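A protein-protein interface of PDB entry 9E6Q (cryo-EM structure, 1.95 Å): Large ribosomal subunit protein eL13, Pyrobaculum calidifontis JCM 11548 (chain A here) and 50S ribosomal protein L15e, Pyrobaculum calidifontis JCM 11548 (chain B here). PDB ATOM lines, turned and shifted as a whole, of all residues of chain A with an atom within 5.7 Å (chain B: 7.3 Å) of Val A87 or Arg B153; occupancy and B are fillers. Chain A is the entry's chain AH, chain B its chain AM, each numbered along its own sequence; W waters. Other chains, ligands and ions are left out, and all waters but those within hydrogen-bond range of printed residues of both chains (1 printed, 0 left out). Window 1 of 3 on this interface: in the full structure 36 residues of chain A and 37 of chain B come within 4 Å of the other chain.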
ATOM      1  N   LYS A  85     -33.837  -1.831 -17.128  1.00  0.00           N
ATOM      2  CA  LYS A  85     -34.603  -1.708 -18.355  1.00  0.00           C
ATOM      3  C   LYS A  85     -33.750  -1.378 -19.567  1.00  0.00           C
ATOM      4  O   LYS A  85     -34.224  -1.532 -20.694  1.00  0.00           O
ATOM      5  CB  LYS A  85     -35.696  -0.644 -18.195  1.00  0.00           C
ATOM      6  CG  LYS A  85     -36.652  -0.925 -17.056  1.00  0.00           C
ATOM      7  CD  LYS A  85     -36.985   0.341 -16.310  1.00  0.00           C
ATOM      8  CE  LYS A  85     -37.769   0.058 -15.051  1.00  0.00           C
ATOM      9  NZ  LYS A  85     -36.960  -0.676 -14.052  1.00  0.00           N
ATOM     10  N   VAL A  86     -32.516  -0.924 -19.371  1.00  0.00           N
ATOM     11  CA  VAL A  86     -31.579  -0.694 -20.458  1.00  0.00           C
ATOM     12  C   VAL A  86     -30.268  -1.379 -20.108  1.00  0.00           C
ATOM     13  O   VAL A  86     -29.981  -1.670 -18.947  1.00  0.00           O
ATOM     14  CB  VAL A  86     -31.339   0.806 -20.737  1.00  0.00           C
ATOM     15  CG1 VAL A  86     -32.638   1.574 -20.723  1.00  0.00           C
ATOM     16  CG2 VAL A  86     -30.376   1.384 -19.731  1.00  0.00           C
ATOM     17  N   VAL A  87     -29.481  -1.656 -21.140  1.00  0.00           N
ATOM     18  CA  VAL A  87     -28.114  -2.130 -20.992  1.00  0.00           C
ATOM     19  C   VAL A  87     -27.252  -1.221 -21.852  1.00  0.00           C
ATOM     20  O   VAL A  87     -27.405  -1.192 -23.076  1.00  0.00           O
ATOM     21  CB  VAL A  87     -27.952  -3.596 -21.404  1.00  0.00           C
ATOM     22  CG1 VAL A  87     -26.490  -3.959 -21.471  1.00  0.00           C
ATOM     23  CG2 VAL A  87     -28.671  -4.495 -20.432  1.00  0.00           C
ATOM     24  N   LYS A  88     -26.348  -0.483 -21.220  1.00  0.00           N
ATOM     25  CA  LYS A  88     -25.562   0.543 -21.895  1.00  0.00           C
ATOM     26  C   LYS A  88     -24.113   0.397 -21.448  1.00  0.00           C
ATOM     27  O   LYS A  88     -23.706   0.984 -20.444  1.00  0.00           O
ATOM     28  CB  LYS A  88     -26.109   1.928 -21.573  1.00  0.00           C
ATOM     29  CG  LYS A  88     -26.106   2.919 -22.715  1.00  0.00           C
ATOM     30  CD  LYS A  88     -24.845   2.867 -23.539  1.00  0.00           C
ATOM     31  CE  LYS A  88     -24.982   3.736 -24.773  1.00  0.00           C
ATOM     32  NZ  LYS A  88     -23.903   3.478 -25.760  1.00  0.00           N
ATOM     33  N   VAL A  89     -23.331  -0.372 -22.195  1.00  0.00           N
ATOM     34  CA  VAL A  89     -21.912  -0.546 -21.924  1.00  0.00           C
ATOM     35  C   VAL A  89     -21.149   0.033 -23.100  1.00  0.00           C
ATOM     36  O   VAL A  89     -21.305  -0.430 -24.234  1.00  0.00           O
ATOM     37  CB  VAL A  89     -21.543  -2.019 -21.707  1.00  0.00           C
ATOM     38  CG1 VAL A  89     -20.061  -2.155 -21.467  1.00  0.00           C
ATOM     39  CG2 VAL A  89     -22.322  -2.581 -20.553  1.00  0.00           C
ATOM     40  N   LYS A  90     -20.318   1.030 -22.833  1.00  0.00           N
ATOM     41  CA  LYS A  90     -19.564   1.683 -23.887  1.00  0.00           C
ATOM     42  C   LYS A  90     -18.234   0.986 -24.108  1.00  0.00           C
ATOM     43  O   LYS A  90     -17.643   0.424 -23.185  1.00  0.00           O
ATOM     44  CB  LYS A  90     -19.316   3.149 -23.550  1.00  0.00           C
ATOM     45  CG  LYS A  90     -20.535   4.024 -23.623  1.00  0.00           C
ATOM     46  CD  LYS A  90     -20.153   5.455 -23.354  1.00  0.00           C
ATOM     47  CE  LYS A  90     -21.361   6.334 -23.202  1.00  0.00           C
ATOM     48  NZ  LYS A  90     -20.999   7.630 -22.593  1.00  0.00           N
ATOM     49  N   ARG A  91     -17.768   1.030 -25.349  1.00  0.00           N
ATOM     50  CA  ARG A  91     -16.433   0.552 -25.661  1.00  0.00           C
ATOM     51  C   ARG A  91     -15.399   1.369 -24.897  1.00  0.00           C
ATOM     52  O   ARG A  91     -15.461   2.599 -24.869  1.00  0.00           O
ATOM     53  CB  ARG A  91     -16.187   0.647 -27.162  1.00  0.00           C
ATOM     54  CG  ARG A  91     -14.738   0.785 -27.535  1.00  0.00           C
ATOM     55  CD  ARG A  91     -14.103  -0.566 -27.700  1.00  0.00           C
ATOM     56  NE  ARG A  91     -12.651  -0.503 -27.612  1.00  0.00           N
ATOM     57  CZ  ARG A  91     -11.840  -0.561 -28.656  1.00  0.00           C
ATOM     58  NH1 ARG A  91     -12.308  -0.652 -29.889  1.00  0.00           N
ATOM     59  NH2 ARG A  91     -10.527  -0.527 -28.458  1.00  0.00           N
ATOM     60  N   GLN B 142     -16.052 -10.075 -29.306  1.00  0.00           N
ATOM     61  CA  GLN B 142     -17.123  -9.114 -29.059  1.00  0.00           C
ATOM     62  C   GLN B 142     -18.269  -9.718 -28.258  1.00  0.00           C
ATOM     63  O   GLN B 142     -18.875  -9.036 -27.429  1.00  0.00           O
ATOM     64  CB  GLN B 142     -17.640  -8.554 -30.382  1.00  0.00           C
ATOM     65  CG  GLN B 142     -16.973  -7.265 -30.783  1.00  0.00           C
ATOM     66  CD  GLN B 142     -16.964  -7.045 -32.276  1.00  0.00           C
ATOM     67  OE1 GLN B 142     -17.264  -7.947 -33.049  1.00  0.00           O
ATOM     68  NE2 GLN B 142     -16.603  -5.839 -32.691  1.00  0.00           N
ATOM     69  N   ASP B 144     -18.157 -12.264 -26.108  1.00  0.00           N
ATOM     70  CA  ASP B 144     -17.782 -12.910 -24.855  1.00  0.00           C
ATOM     71  C   ASP B 144     -18.368 -12.150 -23.668  1.00  0.00           C
ATOM     72  O   ASP B 144     -18.261 -10.922 -23.613  1.00  0.00           O
ATOM     73  CB  ASP B 144     -16.265 -12.987 -24.746  1.00  0.00           C
ATOM     74  CG  ASP B 144     -15.803 -13.664 -23.478  1.00  0.00           C
ATOM     75  OD1 ASP B 144     -15.624 -12.966 -22.463  1.00  0.00           O
ATOM     76  OD2 ASP B 144     -15.613 -14.894 -23.494  1.00  0.00           O
ATOM     77  N   PRO B 145     -18.987 -12.837 -22.704  1.00  0.00           N
ATOM     78  CA  PRO B 145     -19.640 -12.122 -21.595  1.00  0.00           C
ATOM     79  C   PRO B 145     -18.702 -11.265 -20.767  1.00  0.00           C
ATOM     80  O   PRO B 145     -19.119 -10.212 -20.275  1.00  0.00           O
ATOM     81  CB  PRO B 145     -20.253 -13.257 -20.764  1.00  0.00           C
ATOM     82  CG  PRO B 145     -19.515 -14.468 -21.162  1.00  0.00           C
ATOM     83  CD  PRO B 145     -19.152 -14.291 -22.588  1.00  0.00           C
ATOM     84  N   SER B 148     -17.123  -8.345 -23.382  1.00  0.00           N
ATOM     85  CA  SER B 148     -18.079  -7.338 -23.822  1.00  0.00           C
ATOM     86  C   SER B 148     -18.114  -6.152 -22.869  1.00  0.00           C
ATOM     87  O   SER B 148     -18.470  -5.043 -23.275  1.00  0.00           O
ATOM     88  CB  SER B 148     -19.468  -7.954 -23.971  1.00  0.00           C
ATOM     89  OG  SER B 148     -20.135  -8.039 -22.728  1.00  0.00           O
ATOM     90  N   GLY B 149     -17.736  -6.357 -21.609  1.00  0.00           N
ATOM     91  CA  GLY B 149     -17.619  -5.239 -20.692  1.00  0.00           C
ATOM     92  C   GLY B 149     -16.542  -4.255 -21.094  1.00  0.00           C
ATOM     93  O   GLY B 149     -16.567  -3.098 -20.673  1.00  0.00           O
ATOM     94  N   ILE B 150     -15.590  -4.691 -21.911  1.00  0.00           N
ATOM     95  CA  ILE B 150     -14.516  -3.832 -22.388  1.00  0.00           C
ATOM     96  C   ILE B 150     -14.833  -3.345 -23.794  1.00  0.00           C
ATOM     97  O   ILE B 150     -14.539  -2.201 -24.149  1.00  0.00           O
ATOM     98  CB  ILE B 150     -13.166  -4.568 -22.353  1.00  0.00           C
ATOM     99  CG1 ILE B 150     -12.971  -5.259 -21.004  1.00  0.00           C
ATOM    100  CG2 ILE B 150     -12.033  -3.623 -22.660  1.00  0.00           C
ATOM    101  CD1 ILE B 150     -12.860  -4.312 -19.842  1.00  0.00           C
ATOM    102  N   CYS B 151     -15.428  -4.212 -24.602  1.00  0.00           N
ATOM    103  CA  CYS B 151     -15.660  -3.932 -26.009  1.00  0.00           C
ATOM    104  C   CYS B 151     -17.013  -3.297 -26.286  1.00  0.00           C
ATOM    105  O   CYS B 151     -17.261  -2.878 -27.419  1.00  0.00           O
ATOM    106  CB  CYS B 151     -15.519  -5.224 -26.815  1.00  0.00           C
ATOM    107  SG  CYS B 151     -13.872  -5.941 -26.692  1.00  0.00           S
ATOM    108  N   GLY B 152     -17.878  -3.199 -25.299  1.00  0.00           N
ATOM    109  CA  GLY B 152     -19.138  -2.527 -25.509  1.00  0.00           C
ATOM    110  C   GLY B 152     -20.279  -3.508 -25.689  1.00  0.00           C
ATOM    111  O   GLY B 152     -20.105  -4.625 -26.187  1.00  0.00           O
ATOM    112  N   ARG B 153     -21.467  -3.084 -25.276  1.00  0.00           N
ATOM    113  CA  ARG B 153     -22.651  -3.920 -25.358  1.00  0.00           C
ATOM    114  C   ARG B 153     -23.878  -3.024 -25.381  1.00  0.00           C
ATOM    115  O   ARG B 153     -23.966  -2.066 -24.613  1.00  0.00           O
ATOM    116  CB  ARG B 153     -22.725  -4.898 -24.184  1.00  0.00           C
ATOM    117  CG  ARG B 153     -23.709  -6.017 -24.406  1.00  0.00           C
ATOM    118  CD  ARG B 153     -23.800  -6.950 -23.225  1.00  0.00           C
ATOM    119  NE  ARG B 153     -24.987  -7.784 -23.329  1.00  0.00           N
ATOM    120  CZ  ARG B 153     -25.894  -7.931 -22.375  1.00  0.00           C
ATOM    121  NH1 ARG B 153     -25.762  -7.340 -21.200  1.00  0.00           N
ATOM    122  NH2 ARG B 153     -26.959  -8.692 -22.606  1.00  0.00           N
ATOM    123  N   GLU B 154     -24.819  -3.348 -26.262  1.00  0.00           N
ATOM    124  CA  GLU B 154     -26.042  -2.573 -26.430  1.00  0.00           C
ATOM    125  C   GLU B 154     -27.212  -3.535 -26.461  1.00  0.00           C
ATOM    126  O   GLU B 154     -27.224  -4.463 -27.272  1.00  0.00           O
ATOM    127  CB  GLU B 154     -26.008  -1.767 -27.729  1.00  0.00           C
ATOM    128  CG  GLU B 154     -25.156  -0.534 -27.694  1.00  0.00           C
ATOM    129  CD  GLU B 154     -25.628   0.457 -26.669  1.00  0.00           C
ATOM    130  OE1 GLU B 154     -26.794   0.897 -26.754  1.00  0.00           O
ATOM    131  OE2 GLU B 154     -24.829   0.796 -25.777  1.00  0.00           O
ATOM    132  N   VAL B 155     -28.197  -3.317 -25.603  1.00  0.00           N
ATOM    133  CA  VAL B 155     -29.456  -4.044 -25.665  1.00  0.00           C
ATOM    134  C   VAL B 155     -30.570  -3.014 -25.786  1.00  0.00           C
ATOM    135  O   VAL B 155     -30.709  -2.153 -24.913  1.00  0.00           O
ATOM    136  CB  VAL B 155     -29.680  -4.951 -24.445  1.00  0.00           C
ATOM    137  CG1 VAL B 155     -30.999  -5.668 -24.572  1.00  0.00           C
ATOM    138  CG2 VAL B 155     -28.552  -5.955 -24.318  1.00  0.00           C
ATOM    139  N   PRO B 156     -31.370  -3.048 -26.850  1.00  0.00           N
ATOM    140  CA  PRO B 156     -32.422  -2.041 -27.021  1.00  0.00           C
ATOM    141  C   PRO B 156     -33.415  -2.066 -25.871  1.00  0.00           C
ATOM    142  O   PRO B 156     -33.768  -3.126 -25.354  1.00  0.00           O
ATOM    143  CB  PRO B 156     -33.090  -2.443 -28.338  1.00  0.00           C
ATOM    144  CG  PRO B 156     -32.144  -3.363 -29.003  1.00  0.00           C
ATOM    145  CD  PRO B 156     -31.352  -4.031 -27.943  1.00  0.00           C
ATOM    146  N   ARG B 157     -33.874  -0.877 -25.477  1.00  0.00           N
ATOM    147  CA  ARG B 157     -34.838  -0.793 -24.388  1.00  0.00           C
ATOM    148  C   ARG B 157     -36.138  -1.495 -24.740  1.00  0.00           C
ATOM    149  O   ARG B 157     -36.825  -2.007 -23.851  1.00  0.00           O
ATOM    150  CB  ARG B 157     -35.105   0.666 -24.025  1.00  0.00           C
ATOM    151  CG  ARG B 157     -35.671   0.853 -22.629  1.00  0.00           C
ATOM    152  CD  ARG B 157     -36.394   2.176 -22.488  1.00  0.00           C
ATOM    153  NE  ARG B 157     -37.835   1.992 -22.369  1.00  0.00           N
ATOM    154  CZ  ARG B 157     -38.504   2.038 -21.226  1.00  0.00           C
ATOM    155  NH1 ARG B 157     -37.892   2.272 -20.077  1.00  0.00           N
ATOM    156  NH2 ARG B 157     -39.819   1.852 -21.234  1.00  0.00           N
ATOM    157  N   ARG B 159     -36.479  -4.276 -26.085  1.00  0.00           N
ATOM    158  CA  ARG B 159     -36.368  -5.705 -25.826  1.00  0.00           C
ATOM    159  C   ARG B 159     -36.582  -6.017 -24.353  1.00  0.00           C
ATOM    160  O   ARG B 159     -37.395  -6.874 -24.001  1.00  0.00           O
ATOM    161  CB  ARG B 159     -35.007  -6.219 -26.283  1.00  0.00           C
ATOM    162  CG  ARG B 159     -34.971  -7.709 -26.478  1.00  0.00           C
ATOM    163  CD  ARG B 159     -33.599  -8.176 -26.871  1.00  0.00           C
ATOM    164  NE  ARG B 159     -33.316  -7.857 -28.261  1.00  0.00           N
ATOM    165  CZ  ARG B 159     -32.120  -7.948 -28.819  1.00  0.00           C
ATOM    166  NH1 ARG B 159     -31.073  -8.379 -28.139  1.00  0.00           N
ATOM    167  NH2 ARG B 159     -31.973  -7.601 -30.092  1.00  0.00           N
ATOM    168  N   LEU B 160     -35.847  -5.336 -23.476  1.00  0.00           N
ATOM    169  CA  LEU B 160     -35.952  -5.628 -22.052  1.00  0.00           C
ATOM    170  C   LEU B 160     -37.298  -5.199 -21.491  1.00  0.00           C
ATOM    171  O   LEU B 160     -37.913  -5.937 -20.717  1.00  0.00           O
ATOM    172  CB  LEU B 160     -34.820  -4.945 -21.289  1.00  0.00           C
ATOM    173  CG  LEU B 160     -33.409  -5.421 -21.618  1.00  0.00           C
ATOM    174  CD1 LEU B 160     -32.396  -4.715 -20.742  1.00  0.00           C
ATOM    175  CD2 LEU B 160     -33.303  -6.915 -21.440  1.00  0.00           C
HETATM  176  O   HOH W   1     -21.973   0.007 -26.708  1.00  0.00           O
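The side-chain amino group of Lys A88 lies within salt-bridge range of the side-chain carboxylate of Glu B154 (2.8 Å).
O of Val A89 lies within hydrogen-bond range of N of Arg B153 (2.9 Å).
The backbone carbonyl oxygen of Val A87 sits at hydrogen-bond distance from the backbone NH of Val B155 (3.4 Å).
OG of Ser B148 is in hydrogen-bond range of O of Pro B145, at 3.4 Å.
Lys A85 touches Arg B157.
Lys A85 touches Leu B160.
Val A87 touches Arg B153 (CG1 to NH1, 3.5 Å).
O of Val A87 touches CA of Glu B154, 3.9 Å away.
CG2 of Val A87 touches CD1 of Leu B160, 3.7 Å away.
O of Ser B148 touches CG1 of Val A89, 3.8 Å away.
CA of Gly B152 touches O of Val A89, at 3.3 Å.
O of Ile B150 touches CA of Arg A91, 3.7 Å away.
CB of Arg A91 touches O of Cys B151, 3.7 Å away.
Arg A91 touches Gly B152.
Printed residues of chain B within 4 Å of Val A86: Arg B157.
Of chain B, only Arg B153, Glu B154, Val B155 and Leu B160 come within 4 Å of Val A87.
Of the printed residues of chain B, Lys A88 touches Glu B154.
Gln B142 touches none of the printed residues of chain A.
Of the printed residues of chain A, Arg B153 touches Val A87 and Val A89.
Pro B156 touches none of the printed residues of chain A.
The nearest residue of chain B that does not touch Val A87 is Pro B156 (5.8 Å).
The nearest printed residue of chain B that does not touch Lys A85 is Pro B156 (4.9 Å).
Of the 7 printed residues of chain A, 7 touch a printed residue of chain B.
Hydrophobic or aromatic side chains of chain A that line the printed part of chain B: Val A86, Val A87 and Val A89.
Along chain A the printed residues that touch a printed residue of chain B span positions 85 to 91.
Among the printed residues, 16 pairs touch across the chains.
Among the printed residues, Asp or Glu carboxylates within 4 Å of a Lys or Arg side-chain nitrogen of the other chain: Lys A88 with Glu B154.
Water W1 lies within hydrogen-bond range of the backbone carbonyl oxygen (O) of Val A89 (2.6 Å), the side-chain carboxylate (OE2) of Glu B154 (3.1 Å) and the backbone NH (N) of Arg B153 (3.4 Å).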
